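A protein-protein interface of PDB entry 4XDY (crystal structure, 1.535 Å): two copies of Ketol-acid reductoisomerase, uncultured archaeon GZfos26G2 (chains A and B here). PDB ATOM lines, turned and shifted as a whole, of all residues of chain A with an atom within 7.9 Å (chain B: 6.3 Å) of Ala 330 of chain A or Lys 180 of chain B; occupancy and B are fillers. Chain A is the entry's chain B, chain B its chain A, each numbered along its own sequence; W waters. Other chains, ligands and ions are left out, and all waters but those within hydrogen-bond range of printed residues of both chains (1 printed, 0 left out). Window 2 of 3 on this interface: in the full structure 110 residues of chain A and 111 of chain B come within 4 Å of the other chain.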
ATOM      1  N   ILE A 325      11.503 -17.632   9.355  1.00  0.00           N
ATOM      2  CA  ILE A 325      11.656 -18.973   8.718  1.00  0.00           C
ATOM      3  C   ILE A 325      12.189 -18.778   7.295  1.00  0.00           C
ATOM      4  O   ILE A 325      13.114 -19.455   6.860  1.00  0.00           O
ATOM      5  CB  ILE A 325      10.251 -19.660   8.719  1.00  0.00           C
ATOM      6  CG1 ILE A 325       9.856 -20.124  10.112  1.00  0.00           C
ATOM      7  CG2 ILE A 325      10.136 -20.738   7.617  1.00  0.00           C
ATOM      8  CD1 ILE A 325       8.426 -20.595  10.254  1.00  0.00           C
ATOM      9  N   ARG A 326      11.612 -17.851   6.528  1.00  0.00           N
ATOM     10  CA  ARG A 326      11.997 -17.725   5.112  1.00  0.00           C
ATOM     11  C   ARG A 326      13.462 -17.213   5.025  1.00  0.00           C
ATOM     12  O   ARG A 326      14.186 -17.578   4.122  1.00  0.00           O
ATOM     13  CB  ARG A 326      11.073 -16.801   4.316  1.00  0.00           C
ATOM     14  CG  ARG A 326       9.610 -17.274   4.232  1.00  0.00           C
ATOM     15  CD  ARG A 326       8.797 -16.364   3.311  1.00  0.00           C
ATOM     16  NE  ARG A 326       8.727 -15.014   3.832  1.00  0.00           N
ATOM     17  CZ  ARG A 326       7.793 -14.540   4.640  1.00  0.00           C
ATOM     18  NH1 ARG A 326       6.793 -15.274   5.100  1.00  0.00           N
ATOM     19  NH2 ARG A 326       7.870 -13.259   5.064  1.00  0.00           N
ATOM     20  N   LYS A 327      13.862 -16.387   5.990  1.00  0.00           N
ATOM     21  CA  LYS A 327      15.227 -15.839   5.962  1.00  0.00           C
ATOM     22  C   LYS A 327      16.244 -17.003   6.157  1.00  0.00           C
ATOM     23  O   LYS A 327      17.304 -16.970   5.600  1.00  0.00           O
ATOM     24  CB  LYS A 327      15.405 -14.793   7.037  1.00  0.00           C
ATOM     25  CG  LYS A 327      16.816 -14.219   7.077  1.00  0.00           C
ATOM     26  CD  LYS A 327      16.861 -12.786   7.600  1.00  0.00           C
ATOM     27  CE  LYS A 327      16.064 -12.606   8.893  1.00  0.00           C
ATOM     28  NZ  LYS A 327      16.822 -11.796   9.895  1.00  0.00           N
ATOM     29  N   LEU A 328      15.871 -18.030   6.913  1.00  0.00           N
ATOM     30  CA  LEU A 328      16.693 -19.215   7.152  1.00  0.00           C
ATOM     31  C   LEU A 328      16.670 -20.287   6.084  1.00  0.00           C
ATOM     32  O   LEU A 328      17.399 -21.266   6.203  1.00  0.00           O
ATOM     33  CB  LEU A 328      16.350 -19.842   8.497  1.00  0.00           C
ATOM     34  CG  LEU A 328      16.510 -18.931   9.741  1.00  0.00           C
ATOM     35  CD1 LEU A 328      15.688 -19.403  10.945  1.00  0.00           C
ATOM     36  CD2 LEU A 328      17.985 -18.757  10.128  1.00  0.00           C
ATOM     37  N   PHE A 329      15.857 -20.143   5.032  1.00  0.00           N
ATOM     38  CA  PHE A 329      15.946 -21.034   3.859  1.00  0.00           C
ATOM     39  C   PHE A 329      17.340 -21.020   3.196  1.00  0.00           C
ATOM     40  O   PHE A 329      17.874 -19.950   2.950  1.00  0.00           O
ATOM     41  CB  PHE A 329      14.902 -20.680   2.803  1.00  0.00           C
ATOM     42  CG  PHE A 329      13.472 -20.946   3.217  1.00  0.00           C
ATOM     43  CD1 PHE A 329      13.164 -21.855   4.166  1.00  0.00           C
ATOM     44  CD2 PHE A 329      12.411 -20.318   2.528  1.00  0.00           C
ATOM     45  CE1 PHE A 329      11.828 -22.133   4.496  1.00  0.00           C
ATOM     46  CE2 PHE A 329      11.089 -20.538   2.898  1.00  0.00           C
ATOM     47  CZ  PHE A 329      10.791 -21.480   3.860  1.00  0.00           C
ATOM     48  N   ALA A 330      17.869 -22.222   2.905  1.00  0.00           N
ATOM     49  CA  ALA A 330      19.030 -22.494   2.008  1.00  0.00           C
ATOM     50  C   ALA A 330      18.802 -22.209   0.503  1.00  0.00           C
ATOM     51  O   ALA A 330      19.619 -22.633  -0.322  1.00  0.00           O
ATOM     52  CB  ALA A 330      19.477 -23.961   2.191  1.00  0.00           C
ATOM     53  N   GLN A 331      17.717 -21.493   0.161  1.00  0.00           N
ATOM     54  CA  GLN A 331      17.252 -21.241  -1.240  1.00  0.00           C
ATOM     55  C   GLN A 331      18.101 -20.184  -1.968  1.00  0.00           C
ATOM     56  O   GLN A 331      19.114 -20.509  -2.589  1.00  0.00           O
ATOM     57  CB  GLN A 331      15.769 -20.793  -1.252  1.00  0.00           C
ATOM     58  CG  GLN A 331      15.197 -20.515  -2.635  1.00  0.00           C
ATOM     59  CD  GLN A 331      13.794 -21.063  -2.822  1.00  0.00           C
ATOM     60  OE1 GLN A 331      13.556 -21.882  -3.714  1.00  0.00           O
ATOM     61  NE2 GLN A 331      12.858 -20.619  -1.997  1.00  0.00           N
ATOM     62  N   LEU B   4      15.774 -27.165  12.560  1.00  0.00           N
ATOM     63  CA  LEU B   4      17.002 -27.823  12.104  1.00  0.00           C
ATOM     64  C   LEU B   4      17.178 -27.710  10.603  1.00  0.00           C
ATOM     65  O   LEU B   4      16.201 -27.902   9.806  1.00  0.00           O
ATOM     66  CB  LEU B   4      16.996 -29.246  12.584  1.00  0.00           C
ATOM     67  CG  LEU B   4      16.751 -29.501  14.052  1.00  0.00           C
ATOM     68  CD1 LEU B   4      16.717 -30.990  14.378  1.00  0.00           C
ATOM     69  CD2 LEU B   4      17.827 -28.839  14.912  1.00  0.00           C
ATOM     70  N   HIS B   5      18.367 -27.256  10.204  1.00  0.00           N
ATOM     71  CA  HIS B   5      18.751 -27.177   8.812  1.00  0.00           C
ATOM     72  C   HIS B   5      19.948 -28.125   8.523  1.00  0.00           C
ATOM     73  O   HIS B   5      20.279 -28.996   9.336  1.00  0.00           O
ATOM     74  CB  HIS B   5      19.028 -25.705   8.415  1.00  0.00           C
ATOM     75  CG  HIS B   5      17.872 -24.766   8.594  1.00  0.00           C
ATOM     76  ND1 HIS B   5      17.656 -24.057   9.747  1.00  0.00           N
ATOM     77  CD2 HIS B   5      16.844 -24.454   7.764  1.00  0.00           C
ATOM     78  CE1 HIS B   5      16.561 -23.326   9.611  1.00  0.00           C
ATOM     79  NE2 HIS B   5      16.050 -23.559   8.415  1.00  0.00           N
ATOM     80  N   ASP B   6      20.499 -28.000   7.319  1.00  0.00           N
ATOM     81  CA  ASP B   6      21.506 -28.931   6.807  1.00  0.00           C
ATOM     82  C   ASP B   6      22.680 -29.032   7.767  1.00  0.00           C
ATOM     83  O   ASP B   6      23.130 -30.119   8.144  1.00  0.00           O
ATOM     84  CB  ASP B   6      22.051 -28.407   5.484  1.00  0.00           C
ATOM     85  CG  ASP B   6      21.256 -28.891   4.264  1.00  0.00           C
ATOM     86  OD1 ASP B   6      20.329 -29.755   4.355  1.00  0.00           O
ATOM     87  OD2 ASP B   6      21.599 -28.384   3.177  1.00  0.00           O
ATOM     88  N   GLY B 148      16.972 -27.969  -6.130  1.00  0.00           N
ATOM     89  CA  GLY B 148      18.053 -27.545  -5.219  1.00  0.00           C
ATOM     90  C   GLY B 148      17.566 -27.049  -3.865  1.00  0.00           C
ATOM     91  O   GLY B 148      18.324 -26.559  -3.043  1.00  0.00           O
ATOM     92  N   PHE B 149      16.263 -27.206  -3.616  1.00  0.00           N
ATOM     93  CA  PHE B 149      15.630 -26.773  -2.367  1.00  0.00           C
ATOM     94  C   PHE B 149      15.039 -28.052  -1.692  1.00  0.00           C
ATOM     95  O   PHE B 149      15.689 -29.151  -1.693  1.00  0.00           O
ATOM     96  CB  PHE B 149      14.665 -25.621  -2.652  1.00  0.00           C
ATOM     97  CG  PHE B 149      14.110 -24.918  -1.425  1.00  0.00           C
ATOM     98  CD1 PHE B 149      14.937 -24.598  -0.328  1.00  0.00           C
ATOM     99  CD2 PHE B 149      12.730 -24.624  -1.336  1.00  0.00           C
ATOM    100  CE1 PHE B 149      14.386 -23.946   0.791  1.00  0.00           C
ATOM    101  CE2 PHE B 149      12.219 -23.985  -0.220  1.00  0.00           C
ATOM    102  CZ  PHE B 149      13.043 -23.664   0.836  1.00  0.00           C
ATOM    103  N   GLY B 150      13.891 -27.907  -1.007  1.00  0.00           N
ATOM    104  CA  GLY B 150      13.409 -28.965  -0.138  1.00  0.00           C
ATOM    105  C   GLY B 150      12.069 -28.490   0.447  1.00  0.00           C
ATOM    106  O   GLY B 150      11.729 -27.331   0.278  1.00  0.00           O
ATOM    107  N   VAL B 151      11.322 -29.395   1.092  1.00  0.00           N
ATOM    108  CA  VAL B 151      10.030 -29.020   1.742  1.00  0.00           C
ATOM    109  C   VAL B 151      10.237 -29.114   3.218  1.00  0.00           C
ATOM    110  O   VAL B 151      11.039 -29.978   3.686  1.00  0.00           O
ATOM    111  CB  VAL B 151       8.840 -29.882   1.249  1.00  0.00           C
ATOM    112  CG1 VAL B 151       8.645 -29.584  -0.224  1.00  0.00           C
ATOM    113  CG2 VAL B 151       9.124 -31.321   1.546  1.00  0.00           C
ATOM    114  N   THR B 173      15.665 -37.084   6.660  1.00  0.00           N
ATOM    115  CA  THR B 173      15.177 -35.774   6.203  1.00  0.00           C
ATOM    116  C   THR B 173      16.248 -34.944   5.573  1.00  0.00           C
ATOM    117  O   THR B 173      16.041 -34.166   4.645  1.00  0.00           O
ATOM    118  CB  THR B 173      14.487 -34.939   7.308  1.00  0.00           C
ATOM    119  OG1 THR B 173      15.465 -34.463   8.258  1.00  0.00           O
ATOM    120  CG2 THR B 173      13.316 -35.723   7.982  1.00  0.00           C
ATOM    121  N   LYS B 174      17.484 -35.162   6.044  1.00  0.00           N
ATOM    122  CA  LYS B 174      18.595 -34.451   5.413  1.00  0.00           C
ATOM    123  C   LYS B 174      18.902 -35.013   4.014  1.00  0.00           C
ATOM    124  O   LYS B 174      19.131 -34.252   3.073  1.00  0.00           O
ATOM    125  CB  LYS B 174      19.857 -34.542   6.302  1.00  0.00           C
ATOM    126  CG  LYS B 174      20.992 -33.738   5.618  1.00  0.00           C
ATOM    127  CD  LYS B 174      22.276 -33.603   6.390  1.00  0.00           C
ATOM    128  CE  LYS B 174      23.208 -32.684   5.562  1.00  0.00           C
ATOM    129  NZ  LYS B 174      24.218 -32.277   6.540  1.00  0.00           N
ATOM    130  N   HIS B 177      16.636 -33.715   1.672  1.00  0.00           N
ATOM    131  CA  HIS B 177      16.829 -32.265   1.524  1.00  0.00           C
ATOM    132  C   HIS B 177      15.729 -31.389   2.162  1.00  0.00           C
ATOM    133  O   HIS B 177      15.619 -30.171   1.881  1.00  0.00           O
ATOM    134  CB  HIS B 177      17.042 -31.867   0.069  1.00  0.00           C
ATOM    135  CG  HIS B 177      18.282 -32.457  -0.573  1.00  0.00           C
ATOM    136  ND1 HIS B 177      18.709 -32.074  -1.823  1.00  0.00           N
ATOM    137  CD2 HIS B 177      19.170 -33.390  -0.146  1.00  0.00           C
ATOM    138  CE1 HIS B 177      19.813 -32.749  -2.141  1.00  0.00           C
ATOM    139  NE2 HIS B 177      20.081 -33.591  -1.170  1.00  0.00           N
ATOM    140  N   TRP B 178      14.935 -31.989   3.034  1.00  0.00           N
ATOM    141  CA  TRP B 178      13.863 -31.242   3.717  1.00  0.00           C
ATOM    142  C   TRP B 178      14.488 -30.242   4.691  1.00  0.00           C
ATOM    143  O   TRP B 178      13.929 -29.233   4.992  1.00  0.00           O
ATOM    144  CB  TRP B 178      12.951 -32.166   4.508  1.00  0.00           C
ATOM    145  CG  TRP B 178      12.170 -33.214   3.716  1.00  0.00           C
ATOM    146  CD1 TRP B 178      12.176 -33.417   2.366  1.00  0.00           C
ATOM    147  CD2 TRP B 178      11.379 -34.254   4.270  1.00  0.00           C
ATOM    148  NE1 TRP B 178      11.444 -34.534   2.033  1.00  0.00           N
ATOM    149  CE2 TRP B 178      10.920 -35.060   3.175  1.00  0.00           C
ATOM    150  CE3 TRP B 178      11.017 -34.609   5.555  1.00  0.00           C
ATOM    151  CZ2 TRP B 178      10.139 -36.200   3.371  1.00  0.00           C
ATOM    152  CZ3 TRP B 178      10.239 -35.722   5.733  1.00  0.00           C
ATOM    153  CH2 TRP B 178       9.812 -36.490   4.641  1.00  0.00           C
ATOM    154  N   THR B 179      15.691 -30.569   5.176  1.00  0.00           N
ATOM    155  CA  THR B 179      16.447 -29.652   6.036  1.00  0.00           C
ATOM    156  C   THR B 179      16.796 -28.350   5.371  1.00  0.00           C
ATOM    157  O   THR B 179      17.042 -27.357   6.074  1.00  0.00           O
ATOM    158  CB  THR B 179      17.773 -30.370   6.513  1.00  0.00           C
ATOM    159  OG1 THR B 179      18.372 -31.051   5.409  1.00  0.00           O
ATOM    160  CG2 THR B 179      17.479 -31.334   7.545  1.00  0.00           C
ATOM    161  N   LYS B 180      16.775 -28.284   4.029  1.00  0.00           N
ATOM    162  CA  LYS B 180      16.984 -27.020   3.381  1.00  0.00           C
ATOM    163  C   LYS B 180      15.866 -26.002   3.670  1.00  0.00           C
ATOM    164  O   LYS B 180      16.074 -24.771   3.724  1.00  0.00           O
ATOM    165  CB  LYS B 180      17.253 -27.189   1.904  1.00  0.00           C
ATOM    166  CG  LYS B 180      18.504 -28.025   1.637  1.00  0.00           C
ATOM    167  CD  LYS B 180      18.793 -28.050   0.171  1.00  0.00           C
ATOM    168  CE  LYS B 180      19.810 -29.101  -0.177  1.00  0.00           C
ATOM    169  NZ  LYS B 180      21.118 -28.727   0.403  1.00  0.00           N
ATOM    170  N   ALA B 181      14.647 -26.506   3.849  1.00  0.00           N
ATOM    171  CA  ALA B 181      13.547 -25.647   4.270  1.00  0.00           C
ATOM    172  C   ALA B 181      13.480 -25.601   5.795  1.00  0.00           C
ATOM    173  O   ALA B 181      13.234 -24.537   6.381  1.00  0.00           O
ATOM    174  CB  ALA B 181      12.210 -26.214   3.697  1.00  0.00           C
ATOM    175  N   GLY B 182      13.661 -26.761   6.421  1.00  0.00           N
ATOM    176  CA  GLY B 182      13.687 -26.851   7.866  1.00  0.00           C
ATOM    177  C   GLY B 182      12.856 -27.954   8.426  1.00  0.00           C
ATOM    178  O   GLY B 182      11.796 -28.317   7.875  1.00  0.00           O
HETATM  179  O   HOH W   1      13.690 -22.261   7.698  1.00  0.00           O
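The side-chain carboxylate (OD2) of Asp 6 of chain B is in salt-bridge range of the side-chain amino group (NZ) of Lys 180 of chain B (2.8 Å).
Of the printed residues of chain B, Phe 329 of chain A touches Phe 149 (3.6 Å), Lys 180 (3.7 Å) and Ala 181 (3.4 Å).
Ala 330 of chain A touches just one residue of chain B: Lys 180.
Of the printed residues of chain B, Gln 331 of chain A touches Phe 149.
Of the printed residues of chain A, His 5 of chain B touches Leu 328.
Of chain A, only Phe 329 and Ala 330 come within 4 Å of Lys 180 of chain B.
Printed residues of chain A within 4 Å of Ala 181 of chain B: Phe 329.
The nearest residue of chain A that does not touch Lys 180 of chain B is Leu 328 of chain A (4.5 Å).
The nearest printed residue of chain B that does not touch Phe 329 of chain A is His 5 of chain B (4.8 Å).
CG of Phe 329 of chain A touches CZ of Phe 149 of chain B, 3.6 Å away.
Phe 329 of chain A touches Lys 180 of chain B (CA to O, 3.7 Å).
CE1 of Phe 329 of chain A touches O of Ala 181 of chain B, at 3.4 Å.
CD2 of Phe 149 of chain B touches OE1 of Gln 331 of chain A, 3.7 Å away.
The backbone carbonyl oxygen (O) of Lys 180 of chain B sits at hydrogen-bond distance from the backbone NH (N) of Ala 330 of chain A.
O of Leu 328 of chain A sits at hydrogen-bond distance from NE2 of His 5 of chain B.
Water W1 lies within hydrogen-bond range of O of Ala 181 of chain B (2.7 Å), NE2 of His 5 of chain B (2.8 Å) and O of Ile 325 of chain A (3.0 Å).
Of the 7 printed residues of chain A, 4 touch a printed residue of chain B.
Of the 15 printed residues of chain B, 4 touch a printed residue of chain A.
Hydrophobic or aromatic side chains of chain B within 4 Å of the printed part of chain A: His 5 and Phe 149.
Among the printed residues, no Asp or Glu carboxylate lies within 4 Å of a Lys or Arg side-chain nitrogen of the other chain.
No position is printed for both chains.
Of the 6 pairs that touch across the chains among the printed residues, none has its exchanged pair printed and touching as well.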
